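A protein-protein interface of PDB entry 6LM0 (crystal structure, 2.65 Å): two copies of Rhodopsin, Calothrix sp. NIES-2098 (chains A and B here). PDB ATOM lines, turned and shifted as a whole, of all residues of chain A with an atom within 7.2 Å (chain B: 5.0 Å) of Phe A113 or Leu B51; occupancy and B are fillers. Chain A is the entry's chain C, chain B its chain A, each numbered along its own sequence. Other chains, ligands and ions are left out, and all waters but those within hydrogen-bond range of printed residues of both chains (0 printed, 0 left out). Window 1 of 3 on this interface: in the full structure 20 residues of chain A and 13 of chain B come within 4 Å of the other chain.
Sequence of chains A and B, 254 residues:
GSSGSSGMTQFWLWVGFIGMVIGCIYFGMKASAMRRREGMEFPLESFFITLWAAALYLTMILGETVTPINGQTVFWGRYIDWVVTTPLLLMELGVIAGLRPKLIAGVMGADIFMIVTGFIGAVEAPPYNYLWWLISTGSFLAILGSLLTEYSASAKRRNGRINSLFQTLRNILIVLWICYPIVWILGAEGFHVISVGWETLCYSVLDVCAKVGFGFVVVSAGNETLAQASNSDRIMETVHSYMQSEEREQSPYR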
ATOM      1  N   VAL A  83      -8.841 -20.319 -14.512  1.00  0.00           N
ATOM      2  CA  VAL A  83      -9.926 -21.234 -14.188  1.00  0.00           C
ATOM      3  C   VAL A  83      -9.484 -22.364 -13.268  1.00  0.00           C
ATOM      4  O   VAL A  83     -10.330 -23.078 -12.724  1.00  0.00           O
ATOM      5  CB  VAL A  83     -10.548 -21.802 -15.485  1.00  0.00           C
ATOM      6  CG1 VAL A  83      -9.766 -23.013 -15.973  1.00  0.00           C
ATOM      7  CG2 VAL A  83     -12.019 -22.146 -15.272  1.00  0.00           C
ATOM      8  N   VAL A 107     -18.562 -20.497  -3.801  1.00  0.00           N
ATOM      9  CA  VAL A 107     -17.632 -19.444  -4.201  1.00  0.00           C
ATOM     10  C   VAL A 107     -16.724 -19.936  -5.321  1.00  0.00           C
ATOM     11  O   VAL A 107     -16.431 -19.199  -6.272  1.00  0.00           O
ATOM     12  CB  VAL A 107     -16.821 -18.955  -2.986  1.00  0.00           C
ATOM     13  CG1 VAL A 107     -15.844 -17.867  -3.403  1.00  0.00           C
ATOM     14  CG2 VAL A 107     -17.753 -18.452  -1.896  1.00  0.00           C
ATOM     15  N   MET A 108     -16.271 -21.188  -5.231  1.00  0.00           N
ATOM     16  CA  MET A 108     -15.450 -21.753  -6.297  1.00  0.00           C
ATOM     17  C   MET A 108     -16.230 -21.839  -7.603  1.00  0.00           C
ATOM     18  O   MET A 108     -15.694 -21.538  -8.676  1.00  0.00           O
ATOM     19  CB  MET A 108     -14.935 -23.133  -5.892  1.00  0.00           C
ATOM     20  CG  MET A 108     -13.902 -23.113  -4.781  1.00  0.00           C
ATOM     21  SD  MET A 108     -13.329 -24.771  -4.372  1.00  0.00           S
ATOM     22  CE  MET A 108     -12.201 -25.083  -5.726  1.00  0.00           C
ATOM     23  N   GLY A 109     -17.498 -22.250  -7.531  1.00  0.00           N
ATOM     24  CA  GLY A 109     -18.312 -22.315  -8.733  1.00  0.00           C
ATOM     25  C   GLY A 109     -18.533 -20.953  -9.361  1.00  0.00           C
ATOM     26  O   GLY A 109     -18.477 -20.806 -10.585  1.00  0.00           O
ATOM     27  N   ALA A 110     -18.786 -19.937  -8.531  1.00  0.00           N
ATOM     28  CA  ALA A 110     -18.916 -18.580  -9.048  1.00  0.00           C
ATOM     29  C   ALA A 110     -17.603 -18.080  -9.634  1.00  0.00           C
ATOM     30  O   ALA A 110     -17.608 -17.284 -10.580  1.00  0.00           O
ATOM     31  CB  ALA A 110     -19.397 -17.639  -7.942  1.00  0.00           C
ATOM     32  N   ASP A 111     -16.473 -18.535  -9.088  1.00  0.00           N
ATOM     33  CA  ASP A 111     -15.176 -18.132  -9.622  1.00  0.00           C
ATOM     34  C   ASP A 111     -14.941 -18.729 -11.002  1.00  0.00           C
ATOM     35  O   ASP A 111     -14.456 -18.040 -11.909  1.00  0.00           O
ATOM     36  CB  ASP A 111     -14.062 -18.543  -8.661  1.00  0.00           C
ATOM     37  CG  ASP A 111     -12.686 -18.157  -9.166  1.00  0.00           C
ATOM     38  OD1 ASP A 111     -12.116 -18.907  -9.987  1.00  0.00           O
ATOM     39  OD2 ASP A 111     -12.175 -17.100  -8.745  1.00  0.00           O
ATOM     40  N   ILE A 112     -15.265 -20.012 -11.178  1.00  0.00           N
ATOM     41  CA  ILE A 112     -15.179 -20.625 -12.499  1.00  0.00           C
ATOM     42  C   ILE A 112     -16.117 -19.920 -13.467  1.00  0.00           C
ATOM     43  O   ILE A 112     -15.777 -19.693 -14.635  1.00  0.00           O
ATOM     44  CB  ILE A 112     -15.478 -22.133 -12.405  1.00  0.00           C
ATOM     45  CG1 ILE A 112     -14.396 -22.834 -11.584  1.00  0.00           C
ATOM     46  CG2 ILE A 112     -15.583 -22.749 -13.792  1.00  0.00           C
ATOM     47  CD1 ILE A 112     -14.789 -24.211 -11.106  1.00  0.00           C
ATOM     48  N   PHE A 113     -17.311 -19.547 -12.993  1.00  0.00           N
ATOM     49  CA  PHE A 113     -18.228 -18.765 -13.814  1.00  0.00           C
ATOM     50  C   PHE A 113     -17.603 -17.437 -14.224  1.00  0.00           C
ATOM     51  O   PHE A 113     -17.793 -16.975 -15.355  1.00  0.00           O
ATOM     52  CB  PHE A 113     -19.535 -18.533 -13.052  1.00  0.00           C
ATOM     53  CG  PHE A 113     -20.557 -17.734 -13.815  1.00  0.00           C
ATOM     54  CD1 PHE A 113     -21.465 -18.364 -14.650  1.00  0.00           C
ATOM     55  CD2 PHE A 113     -20.619 -16.354 -13.684  1.00  0.00           C
ATOM     56  CE1 PHE A 113     -22.409 -17.633 -15.349  1.00  0.00           C
ATOM     57  CE2 PHE A 113     -21.560 -15.619 -14.381  1.00  0.00           C
ATOM     58  CZ  PHE A 113     -22.456 -16.259 -15.214  1.00  0.00           C
ATOM     59  N   MET A 114     -16.848 -16.814 -13.318  1.00  0.00           N
ATOM     60  CA  MET A 114     -16.235 -15.523 -13.615  1.00  0.00           C
ATOM     61  C   MET A 114     -15.185 -15.651 -14.712  1.00  0.00           C
ATOM     62  O   MET A 114     -15.141 -14.836 -15.642  1.00  0.00           O
ATOM     63  CB  MET A 114     -15.621 -14.936 -12.344  1.00  0.00           C
ATOM     64  CG  MET A 114     -14.981 -13.572 -12.527  1.00  0.00           C
ATOM     65  SD  MET A 114     -13.594 -13.309 -11.406  1.00  0.00           S
ATOM     66  CE  MET A 114     -14.389 -13.537  -9.825  1.00  0.00           C
ATOM     67  N   ILE A 115     -14.331 -16.671 -14.623  1.00  0.00           N
ATOM     68  CA  ILE A 115     -13.273 -16.845 -15.614  1.00  0.00           C
ATOM     69  C   ILE A 115     -13.860 -17.231 -16.966  1.00  0.00           C
ATOM     70  O   ILE A 115     -13.412 -16.749 -18.013  1.00  0.00           O
ATOM     71  CB  ILE A 115     -12.249 -17.886 -15.126  1.00  0.00           C
ATOM     72  CG1 ILE A 115     -11.703 -17.495 -13.751  1.00  0.00           C
ATOM     73  CG2 ILE A 115     -11.117 -18.040 -16.131  1.00  0.00           C
ATOM     74  CD1 ILE A 115     -11.137 -16.093 -13.693  1.00  0.00           C
ATOM     75  N   VAL A 116     -14.874 -18.100 -16.966  1.00  0.00           N
ATOM     76  CA  VAL A 116     -15.437 -18.590 -18.221  1.00  0.00           C
ATOM     77  C   VAL A 116     -16.101 -17.453 -18.991  1.00  0.00           C
ATOM     78  O   VAL A 116     -15.856 -17.268 -20.188  1.00  0.00           O
ATOM     79  CB  VAL A 116     -16.420 -19.744 -17.952  1.00  0.00           C
ATOM     80  CG1 VAL A 116     -17.310 -19.982 -19.161  1.00  0.00           C
ATOM     81  CG2 VAL A 116     -15.657 -21.013 -17.592  1.00  0.00           C
ATOM     82  N   THR A 117     -16.946 -16.670 -18.314  1.00  0.00           N
ATOM     83  CA  THR A 117     -17.589 -15.542 -18.981  1.00  0.00           C
ATOM     84  C   THR A 117     -16.576 -14.478 -19.386  1.00  0.00           C
ATOM     85  O   THR A 117     -16.798 -13.753 -20.362  1.00  0.00           O
ATOM     86  CB  THR A 117     -18.667 -14.937 -18.080  1.00  0.00           C
ATOM     87  OG1 THR A 117     -18.135 -14.733 -16.764  1.00  0.00           O
ATOM     88  CG2 THR A 117     -19.871 -15.867 -17.998  1.00  0.00           C
ATOM     89  N   GLY A 118     -15.464 -14.371 -18.656  1.00  0.00           N
ATOM     90  CA  GLY A 118     -14.407 -13.464 -19.069  1.00  0.00           C
ATOM     91  C   GLY A 118     -13.685 -13.949 -20.312  1.00  0.00           C
ATOM     92  O   GLY A 118     -13.270 -13.146 -21.153  1.00  0.00           O
ATOM     93  N   PHE A 119     -13.523 -15.266 -20.445  1.00  0.00           N
ATOM     94  CA  PHE A 119     -12.922 -15.815 -21.655  1.00  0.00           C
ATOM     95  C   PHE A 119     -13.818 -15.583 -22.865  1.00  0.00           C
ATOM     96  O   PHE A 119     -13.327 -15.301 -23.965  1.00  0.00           O
ATOM     97  CB  PHE A 119     -12.637 -17.305 -21.471  1.00  0.00           C
ATOM     98  CG  PHE A 119     -12.369 -18.035 -22.757  1.00  0.00           C
ATOM     99  CD1 PHE A 119     -13.352 -18.812 -23.346  1.00  0.00           C
ATOM    100  CD2 PHE A 119     -11.132 -17.943 -23.375  1.00  0.00           C
ATOM    101  CE1 PHE A 119     -13.111 -19.482 -24.528  1.00  0.00           C
ATOM    102  CE2 PHE A 119     -10.884 -18.612 -24.558  1.00  0.00           C
ATOM    103  CZ  PHE A 119     -11.875 -19.382 -25.136  1.00  0.00           C
ATOM    104  N   TRP A 132     -20.222  -9.410 -21.783  1.00  0.00           N
ATOM    105  CA  TRP A 132     -19.688 -10.506 -20.982  1.00  0.00           C
ATOM    106  C   TRP A 132     -18.771  -9.995 -19.878  1.00  0.00           C
ATOM    107  O   TRP A 132     -18.641 -10.645 -18.834  1.00  0.00           O
ATOM    108  CB  TRP A 132     -18.953 -11.502 -21.880  1.00  0.00           C
ATOM    109  CG  TRP A 132     -19.877 -12.348 -22.705  1.00  0.00           C
ATOM    110  CD1 TRP A 132     -20.067 -12.278 -24.054  1.00  0.00           C
ATOM    111  CD2 TRP A 132     -20.741 -13.389 -22.231  1.00  0.00           C
ATOM    112  NE1 TRP A 132     -20.994 -13.212 -24.451  1.00  0.00           N
ATOM    113  CE2 TRP A 132     -21.423 -13.906 -23.350  1.00  0.00           C
ATOM    114  CE3 TRP A 132     -21.002 -13.934 -20.970  1.00  0.00           C
ATOM    115  CZ2 TRP A 132     -22.349 -14.943 -23.247  1.00  0.00           C
ATOM    116  CZ3 TRP A 132     -21.924 -14.963 -20.870  1.00  0.00           C
ATOM    117  CH2 TRP A 132     -22.586 -15.456 -22.001  1.00  0.00           C
ATOM    118  N   ILE A 135     -21.142  -9.213 -17.111  1.00  0.00           N
ATOM    119  CA  ILE A 135     -21.641 -10.453 -16.520  1.00  0.00           C
ATOM    120  C   ILE A 135     -20.591 -11.054 -15.594  1.00  0.00           C
ATOM    121  O   ILE A 135     -20.894 -11.473 -14.469  1.00  0.00           O
ATOM    122  CB  ILE A 135     -22.052 -11.443 -17.625  1.00  0.00           C
ATOM    123  CG1 ILE A 135     -23.346 -10.984 -18.299  1.00  0.00           C
ATOM    124  CG2 ILE A 135     -22.206 -12.847 -17.059  1.00  0.00           C
ATOM    125  CD1 ILE A 135     -23.508 -11.501 -19.709  1.00  0.00           C
ATOM    126  N   SER A 136     -19.340 -11.101 -16.055  1.00  0.00           N
ATOM    127  CA  SER A 136     -18.270 -11.664 -15.237  1.00  0.00           C
ATOM    128  C   SER A 136     -17.994 -10.797 -14.014  1.00  0.00           C
ATOM    129  O   SER A 136     -17.773 -11.317 -12.915  1.00  0.00           O
ATOM    130  CB  SER A 136     -17.003 -11.827 -16.075  1.00  0.00           C
ATOM    131  OG  SER A 136     -16.060 -12.659 -15.422  1.00  0.00           O
ATOM    132  N   THR A 137     -18.005  -9.472 -14.183  1.00  0.00           N
ATOM    133  CA  THR A 137     -17.790  -8.580 -13.047  1.00  0.00           C
ATOM    134  C   THR A 137     -18.916  -8.697 -12.029  1.00  0.00           C
ATOM    135  O   THR A 137     -18.693  -8.490 -10.830  1.00  0.00           O
ATOM    136  CB  THR A 137     -17.647  -7.135 -13.533  1.00  0.00           C
ATOM    137  OG1 THR A 137     -16.720  -7.086 -14.624  1.00  0.00           O
ATOM    138  CG2 THR A 137     -17.143  -6.236 -12.412  1.00  0.00           C
ATOM    139  N   GLY A 138     -20.125  -9.036 -12.481  1.00  0.00           N
ATOM    140  CA  GLY A 138     -21.218  -9.255 -11.547  1.00  0.00           C
ATOM    141  C   GLY A 138     -20.937 -10.395 -10.587  1.00  0.00           C
ATOM    142  O   GLY A 138     -21.135 -10.270  -9.376  1.00  0.00           O
ATOM    143  N   SER A 139     -20.464 -11.527 -11.117  1.00  0.00           N
ATOM    144  CA  SER A 139     -20.090 -12.638 -10.248  1.00  0.00           C
ATOM    145  C   SER A 139     -18.874 -12.293  -9.398  1.00  0.00           C
ATOM    146  O   SER A 139     -18.724 -12.820  -8.290  1.00  0.00           O
ATOM    147  CB  SER A 139     -19.824 -13.894 -11.077  1.00  0.00           C
ATOM    148  OG  SER A 139     -18.918 -13.632 -12.133  1.00  0.00           O
ATOM    149  N   PHE A 140     -18.002 -11.413  -9.897  1.00  0.00           N
ATOM    150  CA  PHE A 140     -16.872 -10.955  -9.098  1.00  0.00           C
ATOM    151  C   PHE A 140     -17.344 -10.176  -7.878  1.00  0.00           C
ATOM    152  O   PHE A 140     -16.794 -10.328  -6.782  1.00  0.00           O
ATOM    153  CB  PHE A 140     -15.941 -10.101  -9.958  1.00  0.00           C
ATOM    154  CG  PHE A 140     -14.765  -9.532  -9.211  1.00  0.00           C
ATOM    155  CD1 PHE A 140     -13.972 -10.340  -8.412  1.00  0.00           C
ATOM    156  CD2 PHE A 140     -14.445  -8.188  -9.322  1.00  0.00           C
ATOM    157  CE1 PHE A 140     -12.887  -9.816  -7.731  1.00  0.00           C
ATOM    158  CE2 PHE A 140     -13.363  -7.660  -8.645  1.00  0.00           C
ATOM    159  CZ  PHE A 140     -12.583  -8.475  -7.848  1.00  0.00           C
ATOM    160  N   ILE A 143     -18.562 -12.537  -5.281  1.00  0.00           N
ATOM    161  CA  ILE A 143     -17.448 -13.199  -4.611  1.00  0.00           C
ATOM    162  C   ILE A 143     -16.807 -12.261  -3.597  1.00  0.00           C
ATOM    163  O   ILE A 143     -16.491 -12.667  -2.471  1.00  0.00           O
ATOM    164  CB  ILE A 143     -16.433 -13.705  -5.649  1.00  0.00           C
ATOM    165  CG1 ILE A 143     -16.987 -14.937  -6.360  1.00  0.00           C
ATOM    166  CG2 ILE A 143     -15.095 -14.019  -4.993  1.00  0.00           C
ATOM    167  CD1 ILE A 143     -16.054 -15.511  -7.380  1.00  0.00           C
ATOM    168  N   CYS B  24     -33.045 -17.840 -11.668  1.00  0.00           N
ATOM    169  CA  CYS B  24     -31.843 -17.363 -10.989  1.00  0.00           C
ATOM    170  C   CYS B  24     -32.192 -16.362  -9.895  1.00  0.00           C
ATOM    171  O   CYS B  24     -31.695 -16.459  -8.767  1.00  0.00           O
ATOM    172  CB  CYS B  24     -30.886 -16.734 -12.001  1.00  0.00           C
ATOM    173  SG  CYS B  24     -29.867 -17.915 -12.894  1.00  0.00           S
ATOM    174  N   PHE B  47     -29.678 -22.607  -8.004  1.00  0.00           N
ATOM    175  CA  PHE B  47     -29.277 -21.322  -8.564  1.00  0.00           C
ATOM    176  C   PHE B  47     -28.173 -21.493  -9.601  1.00  0.00           C
ATOM    177  O   PHE B  47     -28.228 -20.899 -10.684  1.00  0.00           O
ATOM    178  CB  PHE B  47     -28.835 -20.388  -7.436  1.00  0.00           C
ATOM    179  CG  PHE B  47     -27.973 -19.248  -7.889  1.00  0.00           C
ATOM    180  CD1 PHE B  47     -28.539 -18.101  -8.421  1.00  0.00           C
ATOM    181  CD2 PHE B  47     -26.594 -19.315  -7.769  1.00  0.00           C
ATOM    182  CE1 PHE B  47     -27.746 -17.050  -8.832  1.00  0.00           C
ATOM    183  CE2 PHE B  47     -25.799 -18.269  -8.181  1.00  0.00           C
ATOM    184  CZ  PHE B  47     -26.374 -17.134  -8.712  1.00  0.00           C
ATOM    185  N   PHE B  48     -27.161 -22.308  -9.290  1.00  0.00           N
ATOM    186  CA  PHE B  48     -26.053 -22.501 -10.220  1.00  0.00           C
ATOM    187  C   PHE B  48     -26.485 -23.266 -11.463  1.00  0.00           C
ATOM    188  O   PHE B  48     -25.934 -23.042 -12.547  1.00  0.00           O
ATOM    189  CB  PHE B  48     -24.901 -23.225  -9.525  1.00  0.00           C
ATOM    190  CG  PHE B  48     -23.942 -22.303  -8.833  1.00  0.00           C
ATOM    191  CD1 PHE B  48     -22.889 -21.732  -9.527  1.00  0.00           C
ATOM    192  CD2 PHE B  48     -24.098 -21.999  -7.491  1.00  0.00           C
ATOM    193  CE1 PHE B  48     -22.006 -20.880  -8.895  1.00  0.00           C
ATOM    194  CE2 PHE B  48     -23.218 -21.147  -6.853  1.00  0.00           C
ATOM    195  CZ  PHE B  48     -22.171 -20.587  -7.557  1.00  0.00           C
ATOM    196  N   ILE B  49     -27.454 -24.173 -11.329  1.00  0.00           N
ATOM    197  CA  ILE B  49     -27.965 -24.896 -12.491  1.00  0.00           C
ATOM    198  C   ILE B  49     -28.633 -23.928 -13.460  1.00  0.00           C
ATOM    199  O   ILE B  49     -28.393 -23.967 -14.672  1.00  0.00           O
ATOM    200  CB  ILE B  49     -28.927 -26.013 -12.048  1.00  0.00           C
ATOM    201  CG1 ILE B  49     -28.142 -27.201 -11.487  1.00  0.00           C
ATOM    202  CG2 ILE B  49     -29.814 -26.449 -13.204  1.00  0.00           C
ATOM    203  CD1 ILE B  49     -28.934 -28.057 -10.516  1.00  0.00           C
ATOM    204  N   THR B  50     -29.472 -23.033 -12.933  1.00  0.00           N
ATOM    205  CA  THR B  50     -30.100 -22.023 -13.779  1.00  0.00           C
ATOM    206  C   THR B  50     -29.094 -20.984 -14.256  1.00  0.00           C
ATOM    207  O   THR B  50     -29.247 -20.435 -15.352  1.00  0.00           O
ATOM    208  CB  THR B  50     -31.246 -21.342 -13.029  1.00  0.00           C
ATOM    209  OG1 THR B  50     -30.772 -20.858 -11.765  1.00  0.00           O
ATOM    210  CG2 THR B  50     -32.390 -22.320 -12.799  1.00  0.00           C
ATOM    211  N   LEU B  51     -28.063 -20.704 -13.454  1.00  0.00           N
ATOM    212  CA  LEU B  51     -27.058 -19.721 -13.848  1.00  0.00           C
ATOM    213  C   LEU B  51     -26.225 -20.226 -15.018  1.00  0.00           C
ATOM    214  O   LEU B  51     -26.008 -19.501 -15.998  1.00  0.00           O
ATOM    215  CB  LEU B  51     -26.163 -19.380 -12.656  1.00  0.00           C
ATOM    216  CG  LEU B  51     -24.982 -18.446 -12.929  1.00  0.00           C
ATOM    217  CD1 LEU B  51     -25.467 -17.071 -13.363  1.00  0.00           C
ATOM    218  CD2 LEU B  51     -24.088 -18.341 -11.702  1.00  0.00           C
ATOM    219  N   TRP B  52     -25.745 -21.468 -14.932  1.00  0.00           N
ATOM    220  CA  TRP B  52     -24.969 -22.039 -16.027  1.00  0.00           C
ATOM    221  C   TRP B  52     -25.808 -22.161 -17.292  1.00  0.00           C
ATOM    222  O   TRP B  52     -25.319 -21.908 -18.399  1.00  0.00           O
ATOM    223  CB  TRP B  52     -24.411 -23.401 -15.616  1.00  0.00           C
ATOM    224  CG  TRP B  52     -23.371 -23.936 -16.552  1.00  0.00           C
ATOM    225  CD1 TRP B  52     -23.507 -24.985 -17.413  1.00  0.00           C
ATOM    226  CD2 TRP B  52     -22.034 -23.449 -16.718  1.00  0.00           C
ATOM    227  NE1 TRP B  52     -22.336 -25.182 -18.107  1.00  0.00           N
ATOM    228  CE2 TRP B  52     -21.417 -24.252 -17.698  1.00  0.00           C
ATOM    229  CE3 TRP B  52     -21.298 -22.414 -16.134  1.00  0.00           C
ATOM    230  CZ2 TRP B  52     -20.100 -24.051 -18.108  1.00  0.00           C
ATOM    231  CZ3 TRP B  52     -19.991 -22.215 -16.541  1.00  0.00           C
ATOM    232  CH2 TRP B  52     -19.406 -23.030 -17.519  1.00  0.00           C
ATOM    233  N   ALA B  53     -27.080 -22.540 -17.147  1.00  0.00           N
ATOM    234  CA  ALA B  53     -27.952 -22.658 -18.309  1.00  0.00           C
ATOM    235  C   ALA B  53     -28.267 -21.293 -18.907  1.00  0.00           C
ATOM    236  O   ALA B  53     -28.353 -21.152 -20.133  1.00  0.00           O
ATOM    237  CB  ALA B  53     -29.240 -23.389 -17.928  1.00  0.00           C
ATOM    238  N   ALA B  54     -28.442 -20.275 -18.058  1.00  0.00           N
ATOM    239  CA  ALA B  54     -28.722 -18.934 -18.561  1.00  0.00           C
ATOM    240  C   ALA B  54     -27.550 -18.392 -19.366  1.00  0.00           C
ATOM    241  O   ALA B  54     -27.744 -17.754 -20.408  1.00  0.00           O
ATOM    242  CB  ALA B  54     -29.055 -17.993 -17.403  1.00  0.00           C
ATOM    243  N   ALA B  55     -26.324 -18.635 -18.901  1.00  0.00           N
ATOM    244  CA  ALA B  55     -25.149 -18.185 -19.640  1.00  0.00           C
ATOM    245  C   ALA B  55     -25.048 -18.891 -20.985  1.00  0.00           C
ATOM    246  O   ALA B  55     -24.889 -18.244 -22.027  1.00  0.00           O
ATOM    247  CB  ALA B  55     -23.887 -18.417 -18.808  1.00  0.00           C
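No position is printed for both chains.
Among the printed residues, merely in contact across the chains: Gly A109 with Phe B48, Ala A110 with Phe B48, Phe A113 with Leu B51, Phe A113 with Ala B55 and Trp A132 with Ala B55.
Phe A113 touches just these residues of chain B: Leu B51 and Ala B55. Leu B51 touches one residue of chain A. Of the printed residues of chain B, Ala A110 touches Phe B48 (3.4 Å). Of the printed residues of chain B, Gly A109 touches Phe B48 (3.5 Å). Of the printed residues of chain A, Ala B55 touches Phe A113 and Trp A132. Of the printed residues of chain A, Phe B48 touches Gly A109 (3.5 Å) and Ala A110 (3.4 Å). Printed residues of chain B within 4 Å of Trp A132: Ala B55 (3.6 Å). Val A107 touches none of the printed residues of chain B. Val A116 touches none of the printed residues of chain B. The nearest printed residue of chain B that does not touch Ala A110 is Leu B51 (5.8 Å).
The side-chain hydroxyl of Thr A117 lies within hydrogen-bond range of the backbone carbonyl oxygen of Phe A113. SG of Cys B24 lies within hydrogen-bond range of N of Leu B51 (3.4 Å).
Of the 10 printed residues of chain B, 3 touch a printed residue of chain A. Hydrophobic or aromatic side chains of chain B that line the printed part of chain A: Phe B48, Leu B51 and Ala B55.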
